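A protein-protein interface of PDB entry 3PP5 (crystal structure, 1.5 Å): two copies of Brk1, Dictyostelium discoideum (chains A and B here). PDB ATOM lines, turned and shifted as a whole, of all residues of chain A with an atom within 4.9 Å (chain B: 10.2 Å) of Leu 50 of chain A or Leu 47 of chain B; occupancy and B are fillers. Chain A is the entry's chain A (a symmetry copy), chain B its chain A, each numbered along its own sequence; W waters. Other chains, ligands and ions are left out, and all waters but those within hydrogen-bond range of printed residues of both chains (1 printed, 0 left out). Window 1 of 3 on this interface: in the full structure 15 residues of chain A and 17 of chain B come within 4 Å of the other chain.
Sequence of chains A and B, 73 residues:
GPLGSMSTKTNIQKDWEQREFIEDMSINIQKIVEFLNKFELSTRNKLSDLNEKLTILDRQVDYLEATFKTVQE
Water W1 bridges the side-chain amide nitrogen of Asn 51 of chain B (2.6 Å) and the side-chain amino group of Lys 53 of chain A (2.8 Å).
Leu 47 of chain B touches its own counterpart, Leu 47 of chain A.
Leu 50 of chain A touches Leu 47 of chain B, but with the chains exchanged Leu 47 of chain A does not touch Leu 50 of chain B (5.7 Å).
Leu 50 of chain A touches Asn 51 of chain B, but with the chains exchanged Asn 51 of chain A does not touch Leu 50 of chain B (8.1 Å).
Lys 53 of chain A touches Leu 54 of chain B, but with the chains exchanged Leu 54 of chain A does not touch Lys 53 of chain B (8.4 Å).
Of the 4 pairs that touch across the chains among the printed residues, 1 has its exchanged pair printed and touching as well.
OD1 of Asn 51 of chain B lies close to O of Leu 47 of chain B.
OD1 of Asn 51 of chain A lies close to O of Leu 47 of chain A, 3.1 Å away.
The backbone carbonyl oxygen of Asn 51 of chain B sits at hydrogen-bond distance from the side-chain hydroxyl of Thr 55 of chain B (2.9 Å).
Printed residues of chain A that touch a printed residue of chain B: Leu 47, Leu 50 and Lys 53.
Among the printed residues, 4 pairs touch across the chains.
Among the printed residues, no Asp or Glu carboxylate lies within 4 Å of a Lys or Arg side-chain nitrogen of the other chain.
Of chain B, only Leu 47 (3.97 Å) comes within 4 Å of Leu 47 of chain A.
Of the printed residues of chain B, Leu 50 of chain A touches Leu 47 (3.6 Å) and Asn 51 (2.9 Å).
Of the printed residues of chain B, Lys 53 of chain A touches Leu 54.
No residue of chain B comes within 4 Å of Leu 54 of chain A.
Arg 44 of chain B touches none of the printed residues of chain A.
Printed residues of chain A within 4 Å of Leu 47 of chain B: Leu 47 and Leu 50.
Of the printed residues of chain A, Asn 51 of chain B touches Leu 50 (2.9 Å).
Of the printed residues of chain A, Leu 54 of chain B touches Lys 53.
Thr 55 of chain B touches none of the printed residues of chain A.
The nearest printed residue of chain A that does not touch Leu 47 of chain B is Lys 46 of chain A (4.1 Å).
CD2 of Leu 47 of chain B touches CD2 of Leu 47 of chain A, 3.97 Å away.
CD2 of Leu 47 of chain B touches CD1 of Leu 50 of chain A, at 3.6 Å.
CD2 of Leu 50 of chain A touches ND2 of Asn 51 of chain B, at 2.9 Å.
CB of Lys 53 of chain A touches CD2 of Leu 54 of chain B, 3.5 Å away.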
ATOM      1  N   LYS A  46      -7.808  -4.681 -28.251  1.00  0.00           N
ATOM      2  CA  LYS A  46      -8.268  -5.351 -27.049  1.00  0.00           C
ATOM      3  C   LYS A  46      -9.616  -6.022 -27.316  1.00  0.00           C
ATOM      4  O   LYS A  46      -9.800  -7.204 -26.971  1.00  0.00           O
ATOM      5  CB  LYS A  46      -8.285  -4.382 -25.856  1.00  0.00           C
ATOM      6  CG  LYS A  46      -6.865  -3.986 -25.422  1.00  0.00           C
ATOM      7  CD  LYS A  46      -6.846  -2.789 -24.472  1.00  0.00           C
ATOM      8  CE  LYS A  46      -5.415  -2.516 -23.997  1.00  0.00           C
ATOM      9  NZ  LYS A  46      -5.287  -1.333 -23.096  1.00  0.00           N
ATOM     10  N   LEU A  47     -10.537  -5.320 -27.975  1.00  0.00           N
ATOM     11  CA  LEU A  47     -11.835  -5.900 -28.323  1.00  0.00           C
ATOM     12  C   LEU A  47     -11.647  -7.129 -29.219  1.00  0.00           C
ATOM     13  O   LEU A  47     -12.331  -8.155 -29.008  1.00  0.00           O
ATOM     14  CB  LEU A  47     -12.726  -4.843 -28.987  1.00  0.00           C
ATOM     15  CG  LEU A  47     -13.188  -3.784 -28.010  1.00  0.00           C
ATOM     16  CD1 LEU A  47     -13.749  -2.573 -28.795  1.00  0.00           C
ATOM     17  CD2 LEU A  47     -14.239  -4.322 -27.062  1.00  0.00           C
ATOM     18  N   SER A  48     -10.728  -7.039 -30.173  1.00  0.00           N
ATOM     19  CA  SER A  48     -10.408  -8.151 -31.057  1.00  0.00           C
ATOM     20  C   SER A  48     -10.043  -9.348 -30.202  1.00  0.00           C
ATOM     21  O   SER A  48     -10.622 -10.447 -30.380  1.00  0.00           O
ATOM     22  CB  SER A  48      -9.231  -7.787 -31.977  1.00  0.00           C
ATOM     23  OG  SER A  48      -8.964  -8.839 -32.894  1.00  0.00           O
ATOM     24  N   ASP A  49      -9.092  -9.137 -29.289  1.00  0.00           N
ATOM     25  CA  ASP A  49      -8.526 -10.224 -28.478  1.00  0.00           C
ATOM     26  C   ASP A  49      -9.617 -10.858 -27.621  1.00  0.00           C
ATOM     27  O   ASP A  49      -9.650 -12.098 -27.490  1.00  0.00           O
ATOM     28  CB  ASP A  49      -7.385  -9.731 -27.583  1.00  0.00           C
ATOM     29  CG  ASP A  49      -6.112  -9.442 -28.357  1.00  0.00           C
ATOM     30  OD1 ASP A  49      -6.055  -9.738 -29.561  1.00  0.00           O
ATOM     31  OD2 ASP A  49      -5.177  -8.881 -27.744  1.00  0.00           O
ATOM     32  N   LEU A  50     -10.497 -10.062 -27.017  1.00  0.00           N
ATOM     33  CA  LEU A  50     -11.590 -10.629 -26.225  1.00  0.00           C
ATOM     34  C   LEU A  50     -12.517 -11.457 -27.084  1.00  0.00           C
ATOM     35  O   LEU A  50     -12.919 -12.577 -26.690  1.00  0.00           O
ATOM     36  CB  LEU A  50     -12.399  -9.561 -25.474  1.00  0.00           C
ATOM     37  CG  LEU A  50     -11.748  -8.960 -24.246  1.00  0.00           C
ATOM     38  CD1 LEU A  50     -12.508  -7.700 -23.807  1.00  0.00           C
ATOM     39  CD2 LEU A  50     -11.772  -9.981 -23.134  1.00  0.00           C
ATOM     40  N   ASN A  51     -12.875 -10.946 -28.252  1.00  0.00           N
ATOM     41  CA  ASN A  51     -13.704 -11.733 -29.168  1.00  0.00           C
ATOM     42  C   ASN A  51     -13.056 -13.049 -29.528  1.00  0.00           C
ATOM     43  O   ASN A  51     -13.731 -14.087 -29.543  1.00  0.00           O
ATOM     44  CB  ASN A  51     -14.008 -10.927 -30.431  1.00  0.00           C
ATOM     45  CG  ASN A  51     -15.169 -10.004 -30.230  1.00  0.00           C
ATOM     46  OD1 ASN A  51     -15.026  -8.762 -30.301  1.00  0.00           O
ATOM     47  ND2 ASN A  51     -16.314 -10.567 -29.910  1.00  0.00           N
ATOM     48  N   GLU A  52     -11.759 -13.025 -29.811  1.00  0.00           N
ATOM     49  CA  GLU A  52     -11.049 -14.256 -30.215  1.00  0.00           C
ATOM     50  C   GLU A  52     -11.076 -15.277 -29.062  1.00  0.00           C
ATOM     51  O   GLU A  52     -11.334 -16.483 -29.258  1.00  0.00           O
ATOM     52  CB  GLU A  52      -9.601 -13.967 -30.600  1.00  0.00           C
ATOM     53  CG  GLU A  52      -8.876 -15.192 -31.031  1.00  0.00           C
ATOM     54  CD  GLU A  52      -7.444 -14.927 -31.455  1.00  0.00           C
ATOM     55  OE1 GLU A  52      -7.054 -13.741 -31.570  1.00  0.00           O
ATOM     56  OE2 GLU A  52      -6.725 -15.918 -31.692  1.00  0.00           O
ATOM     57  N   LYS A  53     -10.825 -14.801 -27.847  1.00  0.00           N
ATOM     58  CA  LYS A  53     -10.836 -15.696 -26.678  1.00  0.00           C
ATOM     59  C   LYS A  53     -12.239 -16.265 -26.463  1.00  0.00           C
ATOM     60  O   LYS A  53     -12.365 -17.470 -26.180  1.00  0.00           O
ATOM     61  CB  LYS A  53     -10.354 -14.977 -25.416  1.00  0.00           C
ATOM     62  CG  LYS A  53      -8.890 -14.584 -25.507  1.00  0.00           C
ATOM     63  CD  LYS A  53      -8.495 -13.720 -24.310  1.00  0.00           C
ATOM     64  CE  LYS A  53      -6.998 -13.423 -24.406  1.00  0.00           C
ATOM     65  NZ  LYS A  53      -6.567 -12.515 -23.292  1.00  0.00           N
ATOM     66  N   LEU A  54     -13.286 -15.460 -26.613  1.00  0.00           N
ATOM     67  CA  LEU A  54     -14.661 -15.966 -26.487  1.00  0.00           C
ATOM     68  C   LEU A  54     -14.957 -16.995 -27.569  1.00  0.00           C
ATOM     69  O   LEU A  54     -15.655 -18.002 -27.302  1.00  0.00           O
ATOM     70  CB  LEU A  54     -15.640 -14.794 -26.584  1.00  0.00           C
ATOM     71  CG  LEU A  54     -17.103 -15.126 -26.531  1.00  0.00           C
ATOM     72  CD1 LEU A  54     -17.423 -15.638 -25.148  1.00  0.00           C
ATOM     73  CD2 LEU A  54     -17.854 -13.824 -26.856  1.00  0.00           C
ATOM     74  N   PHE B  39     -13.225   8.689 -20.024  1.00  0.00           N
ATOM     75  CA  PHE B  39     -13.593   7.637 -20.974  1.00  0.00           C
ATOM     76  C   PHE B  39     -12.500   6.583 -21.072  1.00  0.00           C
ATOM     77  O   PHE B  39     -12.804   5.365 -21.158  1.00  0.00           O
ATOM     78  CB  PHE B  39     -13.916   8.271 -22.340  1.00  0.00           C
ATOM     79  CG  PHE B  39     -14.278   7.287 -23.407  1.00  0.00           C
ATOM     80  CD1 PHE B  39     -15.422   6.506 -23.290  1.00  0.00           C
ATOM     81  CD2 PHE B  39     -13.511   7.169 -24.527  1.00  0.00           C
ATOM     82  CE1 PHE B  39     -15.757   5.637 -24.290  1.00  0.00           C
ATOM     83  CE2 PHE B  39     -13.850   6.280 -25.515  1.00  0.00           C
ATOM     84  CZ  PHE B  39     -14.971   5.521 -25.378  1.00  0.00           C
ATOM     85  N   GLU B  40     -11.239   6.979 -21.008  1.00  0.00           N
ATOM     86  CA  GLU B  40     -10.145   5.993 -21.009  1.00  0.00           C
ATOM     87  C   GLU B  40     -10.257   5.115 -19.773  1.00  0.00           C
ATOM     88  O   GLU B  40     -10.112   3.892 -19.869  1.00  0.00           O
ATOM     89  CB  GLU B  40      -8.757   6.680 -21.066  1.00  0.00           C
ATOM     90  CG  GLU B  40      -7.582   5.702 -21.207  1.00  0.00           C
ATOM     91  CD  GLU B  40      -7.168   5.059 -19.892  1.00  0.00           C
ATOM     92  OE1 GLU B  40      -7.440   5.622 -18.818  1.00  0.00           O
ATOM     93  OE2 GLU B  40      -6.557   3.964 -19.934  1.00  0.00           O
ATOM     94  N   LEU B  41     -10.576   5.710 -18.622  1.00  0.00           N
ATOM     95  CA  LEU B  41     -10.667   4.951 -17.363  1.00  0.00           C
ATOM     96  C   LEU B  41     -11.846   3.998 -17.419  1.00  0.00           C
ATOM     97  O   LEU B  41     -11.726   2.797 -17.062  1.00  0.00           O
ATOM     98  CB  LEU B  41     -10.855   5.915 -16.175  1.00  0.00           C
ATOM     99  CG  LEU B  41     -10.986   5.220 -14.816  1.00  0.00           C
ATOM    100  CD1 LEU B  41      -9.751   4.371 -14.572  1.00  0.00           C
ATOM    101  CD2 LEU B  41     -11.171   6.279 -13.720  1.00  0.00           C
ATOM    102  N   SER B  42     -12.987   4.519 -17.845  1.00  0.00           N
ATOM    103  CA  SER B  42     -14.197   3.719 -17.973  1.00  0.00           C
ATOM    104  C   SER B  42     -13.955   2.501 -18.860  1.00  0.00           C
ATOM    105  O   SER B  42     -14.269   1.356 -18.476  1.00  0.00           O
ATOM    106  CB  SER B  42     -15.331   4.570 -18.542  1.00  0.00           C
ATOM    107  OG  SER B  42     -16.489   3.791 -18.773  1.00  0.00           O
ATOM    108  N   THR B  43     -13.404   2.744 -20.042  1.00  0.00           N
ATOM    109  CA  THR B  43     -13.185   1.711 -21.039  1.00  0.00           C
ATOM    110  C   THR B  43     -12.222   0.669 -20.487  1.00  0.00           C
ATOM    111  O   THR B  43     -12.439  -0.561 -20.608  1.00  0.00           O
ATOM    112  CB  THR B  43     -12.630   2.327 -22.334  1.00  0.00           C
ATOM    113  OG1 THR B  43     -13.623   3.214 -22.840  1.00  0.00           O
ATOM    114  CG2 THR B  43     -12.336   1.233 -23.403  1.00  0.00           C
ATOM    115  N   ARG B  44     -11.157   1.120 -19.843  1.00  0.00           N
ATOM    116  CA  ARG B  44     -10.163   0.219 -19.273  1.00  0.00           C
ATOM    117  C   ARG B  44     -10.819  -0.665 -18.220  1.00  0.00           C
ATOM    118  O   ARG B  44     -10.586  -1.901 -18.182  1.00  0.00           O
ATOM    119  CB  ARG B  44      -9.003   1.050 -18.684  1.00  0.00           C
ATOM    120  CG  ARG B  44      -8.007   0.266 -17.851  1.00  0.00           C
ATOM    121  CD  ARG B  44      -6.606   0.905 -17.876  1.00  0.00           C
ATOM    122  NE  ARG B  44      -6.632   2.362 -17.693  1.00  0.00           N
ATOM    123  CZ  ARG B  44      -6.735   2.967 -16.512  1.00  0.00           C
ATOM    124  NH1 ARG B  44      -6.817   2.248 -15.399  1.00  0.00           N
ATOM    125  NH2 ARG B  44      -6.750   4.294 -16.441  1.00  0.00           N
ATOM    126  N   ASN B  45     -11.677  -0.089 -17.392  1.00  0.00           N
ATOM    127  CA  ASN B  45     -12.333  -0.883 -16.335  1.00  0.00           C
ATOM    128  C   ASN B  45     -13.311  -1.894 -16.919  1.00  0.00           C
ATOM    129  O   ASN B  45     -13.400  -3.043 -16.427  1.00  0.00           O
ATOM    130  CB  ASN B  45     -13.057   0.015 -15.332  1.00  0.00           C
ATOM    131  CG  ASN B  45     -12.084   0.790 -14.437  1.00  0.00           C
ATOM    132  OD1 ASN B  45     -10.905   0.435 -14.334  1.00  0.00           O
ATOM    133  ND2 ASN B  45     -12.578   1.841 -13.788  1.00  0.00           N
ATOM    134  N   LYS B  46     -14.062  -1.485 -17.930  1.00  0.00           N
ATOM    135  CA  LYS B  46     -15.013  -2.392 -18.544  1.00  0.00           C
ATOM    136  C   LYS B  46     -14.268  -3.562 -19.188  1.00  0.00           C
ATOM    137  O   LYS B  46     -14.647  -4.729 -18.982  1.00  0.00           O
ATOM    138  CB  LYS B  46     -15.939  -1.639 -19.513  1.00  0.00           C
ATOM    139  CG  LYS B  46     -16.899  -0.698 -18.768  1.00  0.00           C
ATOM    140  CD  LYS B  46     -17.596   0.296 -19.697  1.00  0.00           C
ATOM    141  CE  LYS B  46     -18.613   1.128 -18.911  1.00  0.00           C
ATOM    142  NZ  LYS B  46     -19.316   2.162 -19.726  1.00  0.00           N
ATOM    143  N   LEU B  47     -13.185  -3.282 -19.913  1.00  0.00           N
ATOM    144  CA  LEU B  47     -12.378  -4.340 -20.522  1.00  0.00           C
ATOM    145  C   LEU B  47     -11.825  -5.276 -19.441  1.00  0.00           C
ATOM    146  O   LEU B  47     -11.844  -6.513 -19.631  1.00  0.00           O
ATOM    147  CB  LEU B  47     -11.258  -3.729 -21.372  1.00  0.00           C
ATOM    148  CG  LEU B  47     -11.783  -3.072 -22.630  1.00  0.00           C
ATOM    149  CD1 LEU B  47     -10.680  -2.168 -23.234  1.00  0.00           C
ATOM    150  CD2 LEU B  47     -12.230  -4.099 -23.648  1.00  0.00           C
ATOM    151  N   SER B  48     -11.373  -4.708 -18.331  1.00  0.00           N
ATOM    152  CA  SER B  48     -10.874  -5.484 -17.203  1.00  0.00           C
ATOM    153  C   SER B  48     -11.949  -6.467 -16.790  1.00  0.00           C
ATOM    154  O   SER B  48     -11.679  -7.689 -16.690  1.00  0.00           O
ATOM    155  CB  SER B  48     -10.529  -4.559 -16.024  1.00  0.00           C
ATOM    156  OG  SER B  48      -9.971  -5.301 -14.948  1.00  0.00           O
ATOM    157  N   ASP B  49     -13.153  -5.941 -16.550  1.00  0.00           N
ATOM    158  CA  ASP B  49     -14.263  -6.735 -16.007  1.00  0.00           C
ATOM    159  C   ASP B  49     -14.626  -7.857 -16.975  1.00  0.00           C
ATOM    160  O   ASP B  49     -14.888  -8.991 -16.527  1.00  0.00           O
ATOM    161  CB  ASP B  49     -15.498  -5.871 -15.731  1.00  0.00           C
ATOM    162  CG  ASP B  49     -15.336  -4.984 -14.510  1.00  0.00           C
ATOM    163  OD1 ASP B  49     -14.331  -5.118 -13.795  1.00  0.00           O
ATOM    164  OD2 ASP B  49     -16.220  -4.126 -14.298  1.00  0.00           O
ATOM    165  N   LEU B  50     -14.670  -7.586 -18.278  1.00  0.00           N
ATOM    166  CA  LEU B  50     -14.964  -8.644 -19.248  1.00  0.00           C
ATOM    167  C   LEU B  50     -13.899  -9.716 -19.229  1.00  0.00           C
ATOM    168  O   LEU B  50     -14.216 -10.928 -19.239  1.00  0.00           O
ATOM    169  CB  LEU B  50     -15.133  -8.111 -20.677  1.00  0.00           C
ATOM    170  CG  LEU B  50     -16.433  -7.395 -20.982  1.00  0.00           C
ATOM    171  CD1 LEU B  50     -16.324  -6.642 -22.316  1.00  0.00           C
ATOM    172  CD2 LEU B  50     -17.542  -8.416 -21.064  1.00  0.00           C
ATOM    173  N   ASN B  51     -12.637  -9.314 -19.199  1.00  0.00           N
ATOM    174  CA  ASN B  51     -11.561 -10.301 -19.095  1.00  0.00           C
ATOM    175  C   ASN B  51     -11.698 -11.160 -17.861  1.00  0.00           C
ATOM    176  O   ASN B  51     -11.522 -12.383 -17.936  1.00  0.00           O
ATOM    177  CB  ASN B  51     -10.200  -9.603 -19.108  1.00  0.00           C
ATOM    178  CG  ASN B  51      -9.746  -9.307 -20.504  1.00  0.00           C
ATOM    179  OD1 ASN B  51      -9.584  -8.128 -20.893  1.00  0.00           O
ATOM    180  ND2 ASN B  51      -9.597 -10.343 -21.302  1.00  0.00           N
ATOM    181  N   GLU B  52     -12.017 -10.543 -16.729  1.00  0.00           N
ATOM    182  CA  GLU B  52     -12.133 -11.295 -15.462  1.00  0.00           C
ATOM    183  C   GLU B  52     -13.276 -12.321 -15.567  1.00  0.00           C
ATOM    184  O   GLU B  52     -13.146 -13.495 -15.162  1.00  0.00           O
ATOM    185  CB  GLU B  52     -12.393 -10.366 -14.281  1.00  0.00           C
ATOM    186  CG  GLU B  52     -12.489 -11.104 -12.994  1.00  0.00           C
ATOM    187  CD  GLU B  52     -12.710 -10.199 -11.795  1.00  0.00           C
ATOM    188  OE1 GLU B  52     -12.627  -8.958 -11.949  1.00  0.00           O
ATOM    189  OE2 GLU B  52     -12.947 -10.748 -10.701  1.00  0.00           O
ATOM    190  N   LYS B  53     -14.404 -11.892 -16.124  1.00  0.00           N
ATOM    191  CA  LYS B  53     -15.553 -12.800 -16.277  1.00  0.00           C
ATOM    192  C   LYS B  53     -15.198 -13.945 -17.226  1.00  0.00           C
ATOM    193  O   LYS B  53     -15.550 -15.102 -16.935  1.00  0.00           O
ATOM    194  CB  LYS B  53     -16.793 -12.056 -16.779  1.00  0.00           C
ATOM    195  CG  LYS B  53     -17.307 -11.053 -15.763  1.00  0.00           C
ATOM    196  CD  LYS B  53     -18.432 -10.213 -16.366  1.00  0.00           C
ATOM    197  CE  LYS B  53     -18.970  -9.280 -15.279  1.00  0.00           C
ATOM    198  NZ  LYS B  53     -20.031  -8.377 -15.835  1.00  0.00           N
ATOM    199  N   LEU B  54     -14.497 -13.673 -18.322  1.00  0.00           N
ATOM    200  CA  LEU B  54     -14.068 -14.742 -19.237  1.00  0.00           C
ATOM    201  C   LEU B  54     -13.110 -15.696 -18.538  1.00  0.00           C
ATOM    202  O   LEU B  54     -13.169 -16.926 -18.772  1.00  0.00           O
ATOM    203  CB  LEU B  54     -13.396 -14.116 -20.462  1.00  0.00           C
ATOM    204  CG  LEU B  54     -12.841 -15.062 -21.488  1.00  0.00           C
ATOM    205  CD1 LEU B  54     -13.993 -15.781 -22.143  1.00  0.00           C
ATOM    206  CD2 LEU B  54     -12.051 -14.199 -22.487  1.00  0.00           C
ATOM    207  N   THR B  55     -12.204 -15.179 -17.710  1.00  0.00           N
ATOM    208  CA  THR B  55     -11.255 -16.044 -16.998  1.00  0.00           C
ATOM    209  C   THR B  55     -11.988 -16.981 -16.024  1.00  0.00           C
ATOM    210  O   THR B  55     -11.677 -18.185 -15.932  1.00  0.00           O
ATOM    211  CB  THR B  55     -10.249 -15.182 -16.251  1.00  0.00           C
ATOM    212  OG1 THR B  55      -9.503 -14.404 -17.206  1.00  0.00           O
ATOM    213  CG2 THR B  55      -9.287 -16.047 -15.443  1.00  0.00           C
HETATM  214  O   HOH W   1      -8.313 -10.380 -23.533  1.00  0.00           O
